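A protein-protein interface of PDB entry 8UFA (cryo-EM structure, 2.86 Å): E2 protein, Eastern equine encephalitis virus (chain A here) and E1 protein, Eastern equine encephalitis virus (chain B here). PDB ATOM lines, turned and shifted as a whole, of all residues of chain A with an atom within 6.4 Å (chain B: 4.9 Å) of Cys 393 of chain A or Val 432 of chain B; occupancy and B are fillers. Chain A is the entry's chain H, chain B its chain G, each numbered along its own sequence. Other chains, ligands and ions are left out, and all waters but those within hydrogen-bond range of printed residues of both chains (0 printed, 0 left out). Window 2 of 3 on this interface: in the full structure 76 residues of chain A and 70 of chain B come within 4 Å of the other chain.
The side-chain hydroxyl (OG1) of Thr 389 of chain A lies within hydrogen-bond range of the side-chain hydroxyl (OG1) of Thr 429 of chain B (3.5 Å).
The side-chain sulfur (SG) of Cys 393 of chain A forms a disulfide with the side-chain sulfur (SG) of Cys 413 of chain A.
Thr 429 of chain B touches Arg 388 of chain A. CG2 of Thr 389 of chain A touches O of Ala 428 of chain B, 3.6 Å away. CG2 of Thr 389 of chain A touches CB of Val 432 of chain B, 3.7 Å away. Val 432 of chain B touches Leu 392 of chain A (CG2 to CB, 3.7 Å). Leu 392 of chain A touches Leu 436 of chain B (O to CD2, 3.9 Å). Cys 393 of chain A touches Val 432 of chain B. Leu 436 of chain B touches Pro 396 of chain A (CD2 to CG, 3.8 Å).
Of the printed residues of chain B, Arg 388 of chain A touches Thr 429 (3.6 Å). Of the printed residues of chain B, Thr 389 of chain A touches Ala 428, Thr 429 and Val 432. Cys 393 of chain A touches one residue of chain B. Cys 413 of chain A touches none of the printed residues of chain B. Of the printed residues of chain A, Ala 428 of chain B touches Thr 389. Of the printed residues of chain A, Thr 429 of chain B touches Arg 388 (3.6 Å) and Thr 389 (3.5 Å). Of chain A, only Thr 389 (3.7 Å), Leu 392 (3.7 Å) and Cys 393 (3.9 Å) come within 4 Å of Val 432 of chain B. Ala 433 of chain B touches none of the printed residues of chain A. The nearest residue of chain A that does not touch Val 432 of chain B is Arg 388 of chain A (5.5 Å).
Of the 14 printed residues of chain A, 5 touch a printed residue of chain B. Hydrophobic or aromatic side chains of chain A within 4 Å of the printed part of chain B: Leu 392 and Pro 396. Of the 9 printed residues of chain B, 4 touch a printed residue of chain A. Printed residues of chain B that touch a printed residue of chain A: Ala 428, Thr 429, Val 432 and Leu 436. Among the printed residues, 8 pairs touch across the chains. Among the printed residues, no Asp or Glu carboxylate lies within 4 Å of a Lys or Arg side-chain nitrogen of the other chain.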
ATOM      1  N   ARG A 388       3.659 -21.240 -29.087  1.00  0.00           N
ATOM      2  CA  ARG A 388       2.756 -22.379 -29.189  1.00  0.00           C
ATOM      3  C   ARG A 388       3.494 -23.673 -28.874  1.00  0.00           C
ATOM      4  O   ARG A 388       2.962 -24.552 -28.185  1.00  0.00           O
ATOM      5  CB  ARG A 388       2.136 -22.429 -30.585  1.00  0.00           C
ATOM      6  CG  ARG A 388       1.176 -23.583 -30.811  1.00  0.00           C
ATOM      7  CD  ARG A 388       0.602 -23.544 -32.217  1.00  0.00           C
ATOM      8  NE  ARG A 388      -0.344 -24.625 -32.462  1.00  0.00           N
ATOM      9  CZ  ARG A 388      -0.011 -25.848 -32.853  1.00  0.00           C
ATOM     10  NH1 ARG A 388       1.243 -26.167 -33.135  1.00  0.00           N
ATOM     11  NH2 ARG A 388      -0.963 -26.765 -32.990  1.00  0.00           N
ATOM     12  N   THR A 389       4.721 -23.809 -29.378  1.00  0.00           N
ATOM     13  CA  THR A 389       5.528 -24.987 -29.080  1.00  0.00           C
ATOM     14  C   THR A 389       5.860 -25.080 -27.594  1.00  0.00           C
ATOM     15  O   THR A 389       5.846 -26.174 -27.018  1.00  0.00           O
ATOM     16  CB  THR A 389       6.812 -24.961 -29.909  1.00  0.00           C
ATOM     17  OG1 THR A 389       6.485 -25.035 -31.302  1.00  0.00           O
ATOM     18  CG2 THR A 389       7.713 -26.127 -29.539  1.00  0.00           C
ATOM     19  N   ARG A 390       6.180 -23.950 -26.959  1.00  0.00           N
ATOM     20  CA  ARG A 390       6.497 -23.975 -25.534  1.00  0.00           C
ATOM     21  C   ARG A 390       5.307 -24.457 -24.713  1.00  0.00           C
ATOM     22  O   ARG A 390       5.453 -25.313 -23.833  1.00  0.00           O
ATOM     23  CB  ARG A 390       6.943 -22.590 -25.063  1.00  0.00           C
ATOM     24  CG  ARG A 390       7.397 -22.557 -23.606  1.00  0.00           C
ATOM     25  CD  ARG A 390       7.977 -21.205 -23.229  1.00  0.00           C
ATOM     26  NE  ARG A 390       8.589 -21.221 -21.905  1.00  0.00           N
ATOM     27  CZ  ARG A 390       7.973 -20.896 -20.776  1.00  0.00           C
ATOM     28  NH1 ARG A 390       6.695 -20.547 -20.758  1.00  0.00           N
ATOM     29  NH2 ARG A 390       8.655 -20.922 -19.635  1.00  0.00           N
ATOM     30  N   ASN A 391       4.114 -23.927 -24.995  1.00  0.00           N
ATOM     31  CA  ASN A 391       2.931 -24.356 -24.258  1.00  0.00           C
ATOM     32  C   ASN A 391       2.669 -25.842 -24.464  1.00  0.00           C
ATOM     33  O   ASN A 391       2.348 -26.560 -23.511  1.00  0.00           O
ATOM     34  CB  ASN A 391       1.717 -23.529 -24.681  1.00  0.00           C
ATOM     35  CG  ASN A 391       1.795 -22.091 -24.199  1.00  0.00           C
ATOM     36  OD1 ASN A 391       2.516 -21.781 -23.251  1.00  0.00           O
ATOM     37  ND2 ASN A 391       1.053 -21.207 -24.857  1.00  0.00           N
ATOM     38  N   LEU A 392       2.802 -26.323 -25.701  1.00  0.00           N
ATOM     39  CA  LEU A 392       2.658 -27.753 -25.947  1.00  0.00           C
ATOM     40  C   LEU A 392       3.733 -28.538 -25.209  1.00  0.00           C
ATOM     41  O   LEU A 392       3.494 -29.663 -24.757  1.00  0.00           O
ATOM     42  CB  LEU A 392       2.739 -28.042 -27.448  1.00  0.00           C
ATOM     43  CG  LEU A 392       1.612 -27.552 -28.358  1.00  0.00           C
ATOM     44  CD1 LEU A 392       1.980 -27.796 -29.813  1.00  0.00           C
ATOM     45  CD2 LEU A 392       0.304 -28.235 -28.018  1.00  0.00           C
ATOM     46  N   CYS A 393       4.931 -27.964 -25.097  1.00  0.00           N
ATOM     47  CA  CYS A 393       6.037 -28.638 -24.423  1.00  0.00           C
ATOM     48  C   CYS A 393       5.812 -28.747 -22.918  1.00  0.00           C
ATOM     49  O   CYS A 393       6.023 -29.814 -22.328  1.00  0.00           O
ATOM     50  CB  CYS A 393       7.339 -27.886 -24.707  1.00  0.00           C
ATOM     51  SG  CYS A 393       8.831 -28.670 -24.048  1.00  0.00           S
ATOM     52  N   ILE A 394       5.386 -27.661 -22.280  1.00  0.00           N
ATOM     53  CA  ILE A 394       5.256 -27.653 -20.825  1.00  0.00           C
ATOM     54  C   ILE A 394       3.898 -28.146 -20.328  1.00  0.00           C
ATOM     55  O   ILE A 394       3.822 -28.734 -19.244  1.00  0.00           O
ATOM     56  CB  ILE A 394       5.558 -26.243 -20.286  1.00  0.00           C
ATOM     57  CG1 ILE A 394       4.448 -25.263 -20.673  1.00  0.00           C
ATOM     58  CG2 ILE A 394       6.906 -25.762 -20.798  1.00  0.00           C
ATOM     59  CD1 ILE A 394       4.670 -23.860 -20.157  1.00  0.00           C
ATOM     60  N   THR A 395       2.824 -27.919 -21.080  1.00  0.00           N
ATOM     61  CA  THR A 395       1.497 -28.317 -20.618  1.00  0.00           C
ATOM     62  C   THR A 395       1.418 -29.776 -20.184  1.00  0.00           C
ATOM     63  O   THR A 395       0.790 -30.047 -19.147  1.00  0.00           O
ATOM     64  CB  THR A 395       0.459 -28.025 -21.712  1.00  0.00           C
ATOM     65  OG1 THR A 395       0.434 -26.620 -21.985  1.00  0.00           O
ATOM     66  CG2 THR A 395      -0.931 -28.464 -21.273  1.00  0.00           C
ATOM     67  N   PRO A 396       2.003 -30.743 -20.893  1.00  0.00           N
ATOM     68  CA  PRO A 396       1.925 -32.137 -20.425  1.00  0.00           C
ATOM     69  C   PRO A 396       2.512 -32.348 -19.044  1.00  0.00           C
ATOM     70  O   PRO A 396       2.178 -33.344 -18.390  1.00  0.00           O
ATOM     71  CB  PRO A 396       2.716 -32.911 -21.488  1.00  0.00           C
ATOM     72  CG  PRO A 396       2.660 -32.058 -22.701  1.00  0.00           C
ATOM     73  CD  PRO A 396       2.667 -30.645 -22.203  1.00  0.00           C
ATOM     74  N   TYR A 397       3.380 -31.451 -18.583  1.00  0.00           N
ATOM     75  CA  TYR A 397       4.002 -31.559 -17.271  1.00  0.00           C
ATOM     76  C   TYR A 397       3.382 -30.637 -16.233  1.00  0.00           C
ATOM     77  O   TYR A 397       3.332 -30.999 -15.053  1.00  0.00           O
ATOM     78  CB  TYR A 397       5.502 -31.278 -17.395  1.00  0.00           C
ATOM     79  CG  TYR A 397       6.196 -32.285 -18.282  1.00  0.00           C
ATOM     80  CD1 TYR A 397       6.606 -33.508 -17.779  1.00  0.00           C
ATOM     81  CD2 TYR A 397       6.432 -32.020 -19.620  1.00  0.00           C
ATOM     82  CE1 TYR A 397       7.248 -34.426 -18.575  1.00  0.00           C
ATOM     83  CE2 TYR A 397       7.065 -32.936 -20.428  1.00  0.00           C
ATOM     84  CZ  TYR A 397       7.466 -34.141 -19.902  1.00  0.00           C
ATOM     85  OH  TYR A 397       8.080 -35.066 -20.709  1.00  0.00           O
ATOM     86  N   LEU A 409      14.200 -30.797 -21.005  1.00  0.00           N
ATOM     87  CA  LEU A 409      13.043 -29.962 -21.308  1.00  0.00           C
ATOM     88  C   LEU A 409      12.931 -28.787 -20.346  1.00  0.00           C
ATOM     89  O   LEU A 409      12.427 -27.724 -20.723  1.00  0.00           O
ATOM     90  CB  LEU A 409      11.762 -30.797 -21.268  1.00  0.00           C
ATOM     91  CG  LEU A 409      11.641 -31.930 -22.290  1.00  0.00           C
ATOM     92  CD1 LEU A 409      10.333 -32.676 -22.097  1.00  0.00           C
ATOM     93  CD2 LEU A 409      11.740 -31.384 -23.705  1.00  0.00           C
ATOM     94  N   LEU A 412      15.424 -26.384 -21.932  1.00  0.00           N
ATOM     95  CA  LEU A 412      15.101 -26.021 -23.306  1.00  0.00           C
ATOM     96  C   LEU A 412      13.772 -25.278 -23.406  1.00  0.00           C
ATOM     97  O   LEU A 412      13.688 -24.235 -24.062  1.00  0.00           O
ATOM     98  CB  LEU A 412      15.076 -27.279 -24.176  1.00  0.00           C
ATOM     99  CG  LEU A 412      14.729 -27.086 -25.654  1.00  0.00           C
ATOM    100  CD1 LEU A 412      15.745 -26.202 -26.350  1.00  0.00           C
ATOM    101  CD2 LEU A 412      14.633 -28.438 -26.335  1.00  0.00           C
ATOM    102  N   CYS A 413      12.726 -25.795 -22.759  1.00  0.00           N
ATOM    103  CA  CYS A 413      11.395 -25.199 -22.833  1.00  0.00           C
ATOM    104  C   CYS A 413      11.124 -24.240 -21.678  1.00  0.00           C
ATOM    105  O   CYS A 413      10.823 -23.065 -21.903  1.00  0.00           O
ATOM    106  CB  CYS A 413      10.327 -26.302 -22.860  1.00  0.00           C
ATOM    107  SG  CYS A 413      10.306 -27.308 -24.367  1.00  0.00           S
ATOM    108  N   CYS A 414      11.222 -24.722 -20.443  1.00  0.00           N
ATOM    109  CA  CYS A 414      10.950 -23.883 -19.284  1.00  0.00           C
ATOM    110  C   CYS A 414      12.042 -22.836 -19.115  1.00  0.00           C
ATOM    111  O   CYS A 414      11.872 -21.680 -19.502  1.00  0.00           O
ATOM    112  CB  CYS A 414      10.828 -24.730 -18.014  1.00  0.00           C
ATOM    113  SG  CYS A 414       9.416 -25.862 -17.987  1.00  0.00           S
ATOM    114  N   ALA B 428      10.501 -26.506 -34.581  1.00  0.00           N
ATOM    115  CA  ALA B 428      10.040 -26.707 -33.213  1.00  0.00           C
ATOM    116  C   ALA B 428       8.627 -27.276 -33.193  1.00  0.00           C
ATOM    117  O   ALA B 428       8.326 -28.185 -32.411  1.00  0.00           O
ATOM    118  CB  ALA B 428      10.099 -25.389 -32.440  1.00  0.00           C
ATOM    119  N   THR B 429       7.753 -26.766 -34.061  1.00  0.00           N
ATOM    120  CA  THR B 429       6.386 -27.269 -34.118  1.00  0.00           C
ATOM    121  C   THR B 429       6.348 -28.732 -34.545  1.00  0.00           C
ATOM    122  O   THR B 429       5.587 -29.530 -33.985  1.00  0.00           O
ATOM    123  CB  THR B 429       5.558 -26.417 -35.081  1.00  0.00           C
ATOM    124  OG1 THR B 429       5.531 -25.060 -34.621  1.00  0.00           O
ATOM    125  CG2 THR B 429       4.137 -26.944 -35.187  1.00  0.00           C
ATOM    126  N   ALA B 430       7.147 -29.100 -35.545  1.00  0.00           N
ATOM    127  CA  ALA B 430       7.163 -30.485 -36.002  1.00  0.00           C
ATOM    128  C   ALA B 430       7.688 -31.431 -34.929  1.00  0.00           C
ATOM    129  O   ALA B 430       7.180 -32.547 -34.776  1.00  0.00           O
ATOM    130  CB  ALA B 430       8.006 -30.606 -37.271  1.00  0.00           C
ATOM    131  N   VAL B 431       8.706 -31.008 -34.179  1.00  0.00           N
ATOM    132  CA  VAL B 431       9.277 -31.867 -33.143  1.00  0.00           C
ATOM    133  C   VAL B 431       8.316 -32.026 -31.970  1.00  0.00           C
ATOM    134  O   VAL B 431       8.119 -33.136 -31.461  1.00  0.00           O
ATOM    135  CB  VAL B 431      10.640 -31.318 -32.687  1.00  0.00           C
ATOM    136  CG1 VAL B 431      11.151 -32.083 -31.474  1.00  0.00           C
ATOM    137  CG2 VAL B 431      11.644 -31.405 -33.821  1.00  0.00           C
ATOM    138  N   VAL B 432       7.708 -30.930 -31.517  1.00  0.00           N
ATOM    139  CA  VAL B 432       6.811 -31.030 -30.368  1.00  0.00           C
ATOM    140  C   VAL B 432       5.588 -31.867 -30.715  1.00  0.00           C
ATOM    141  O   VAL B 432       5.090 -32.634 -29.883  1.00  0.00           O
ATOM    142  CB  VAL B 432       6.419 -29.628 -29.864  1.00  0.00           C
ATOM    143  CG1 VAL B 432       5.431 -28.961 -30.809  1.00  0.00           C
ATOM    144  CG2 VAL B 432       5.848 -29.722 -28.456  1.00  0.00           C
ATOM    145  N   ALA B 433       5.087 -31.747 -31.944  1.00  0.00           N
ATOM    146  CA  ALA B 433       3.965 -32.582 -32.357  1.00  0.00           C
ATOM    147  C   ALA B 433       4.336 -34.058 -32.293  1.00  0.00           C
ATOM    148  O   ALA B 433       3.516 -34.898 -31.908  1.00  0.00           O
ATOM    149  CB  ALA B 433       3.519 -32.200 -33.767  1.00  0.00           C
ATOM    150  N   LEU B 434       5.568 -34.390 -32.673  1.00  0.00           N
ATOM    151  CA  LEU B 434       6.031 -35.771 -32.587  1.00  0.00           C
ATOM    152  C   LEU B 434       6.213 -36.209 -31.138  1.00  0.00           C
ATOM    153  O   LEU B 434       5.913 -37.357 -30.790  1.00  0.00           O
ATOM    154  CB  LEU B 434       7.335 -35.922 -33.368  1.00  0.00           C
ATOM    155  CG  LEU B 434       7.961 -37.313 -33.416  1.00  0.00           C
ATOM    156  CD1 LEU B 434       7.015 -38.316 -34.043  1.00  0.00           C
ATOM    157  CD2 LEU B 434       9.264 -37.245 -34.192  1.00  0.00           C
ATOM    158  N   VAL B 435       6.704 -35.314 -30.280  1.00  0.00           N
ATOM    159  CA  VAL B 435       6.872 -35.652 -28.868  1.00  0.00           C
ATOM    160  C   VAL B 435       5.529 -36.006 -28.244  1.00  0.00           C
ATOM    161  O   VAL B 435       5.415 -36.987 -27.498  1.00  0.00           O
ATOM    162  CB  VAL B 435       7.558 -34.492 -28.123  1.00  0.00           C
ATOM    163  CG1 VAL B 435       7.486 -34.698 -26.617  1.00  0.00           C
ATOM    164  CG2 VAL B 435       9.004 -34.366 -28.569  1.00  0.00           C
ATOM    165  N   LEU B 436       4.493 -35.219 -28.537  1.00  0.00           N
ATOM    166  CA  LEU B 436       3.163 -35.537 -28.025  1.00  0.00           C
ATOM    167  C   LEU B 436       2.682 -36.879 -28.555  1.00  0.00           C
ATOM    168  O   LEU B 436       2.002 -37.629 -27.845  1.00  0.00           O
ATOM    169  CB  LEU B 436       2.177 -34.432 -28.402  1.00  0.00           C
ATOM    170  CG  LEU B 436       2.484 -33.039 -27.851  1.00  0.00           C
ATOM    171  CD1 LEU B 436       1.508 -32.022 -28.419  1.00  0.00           C
ATOM    172  CD2 LEU B 436       2.443 -33.038 -26.331  1.00  0.00           C
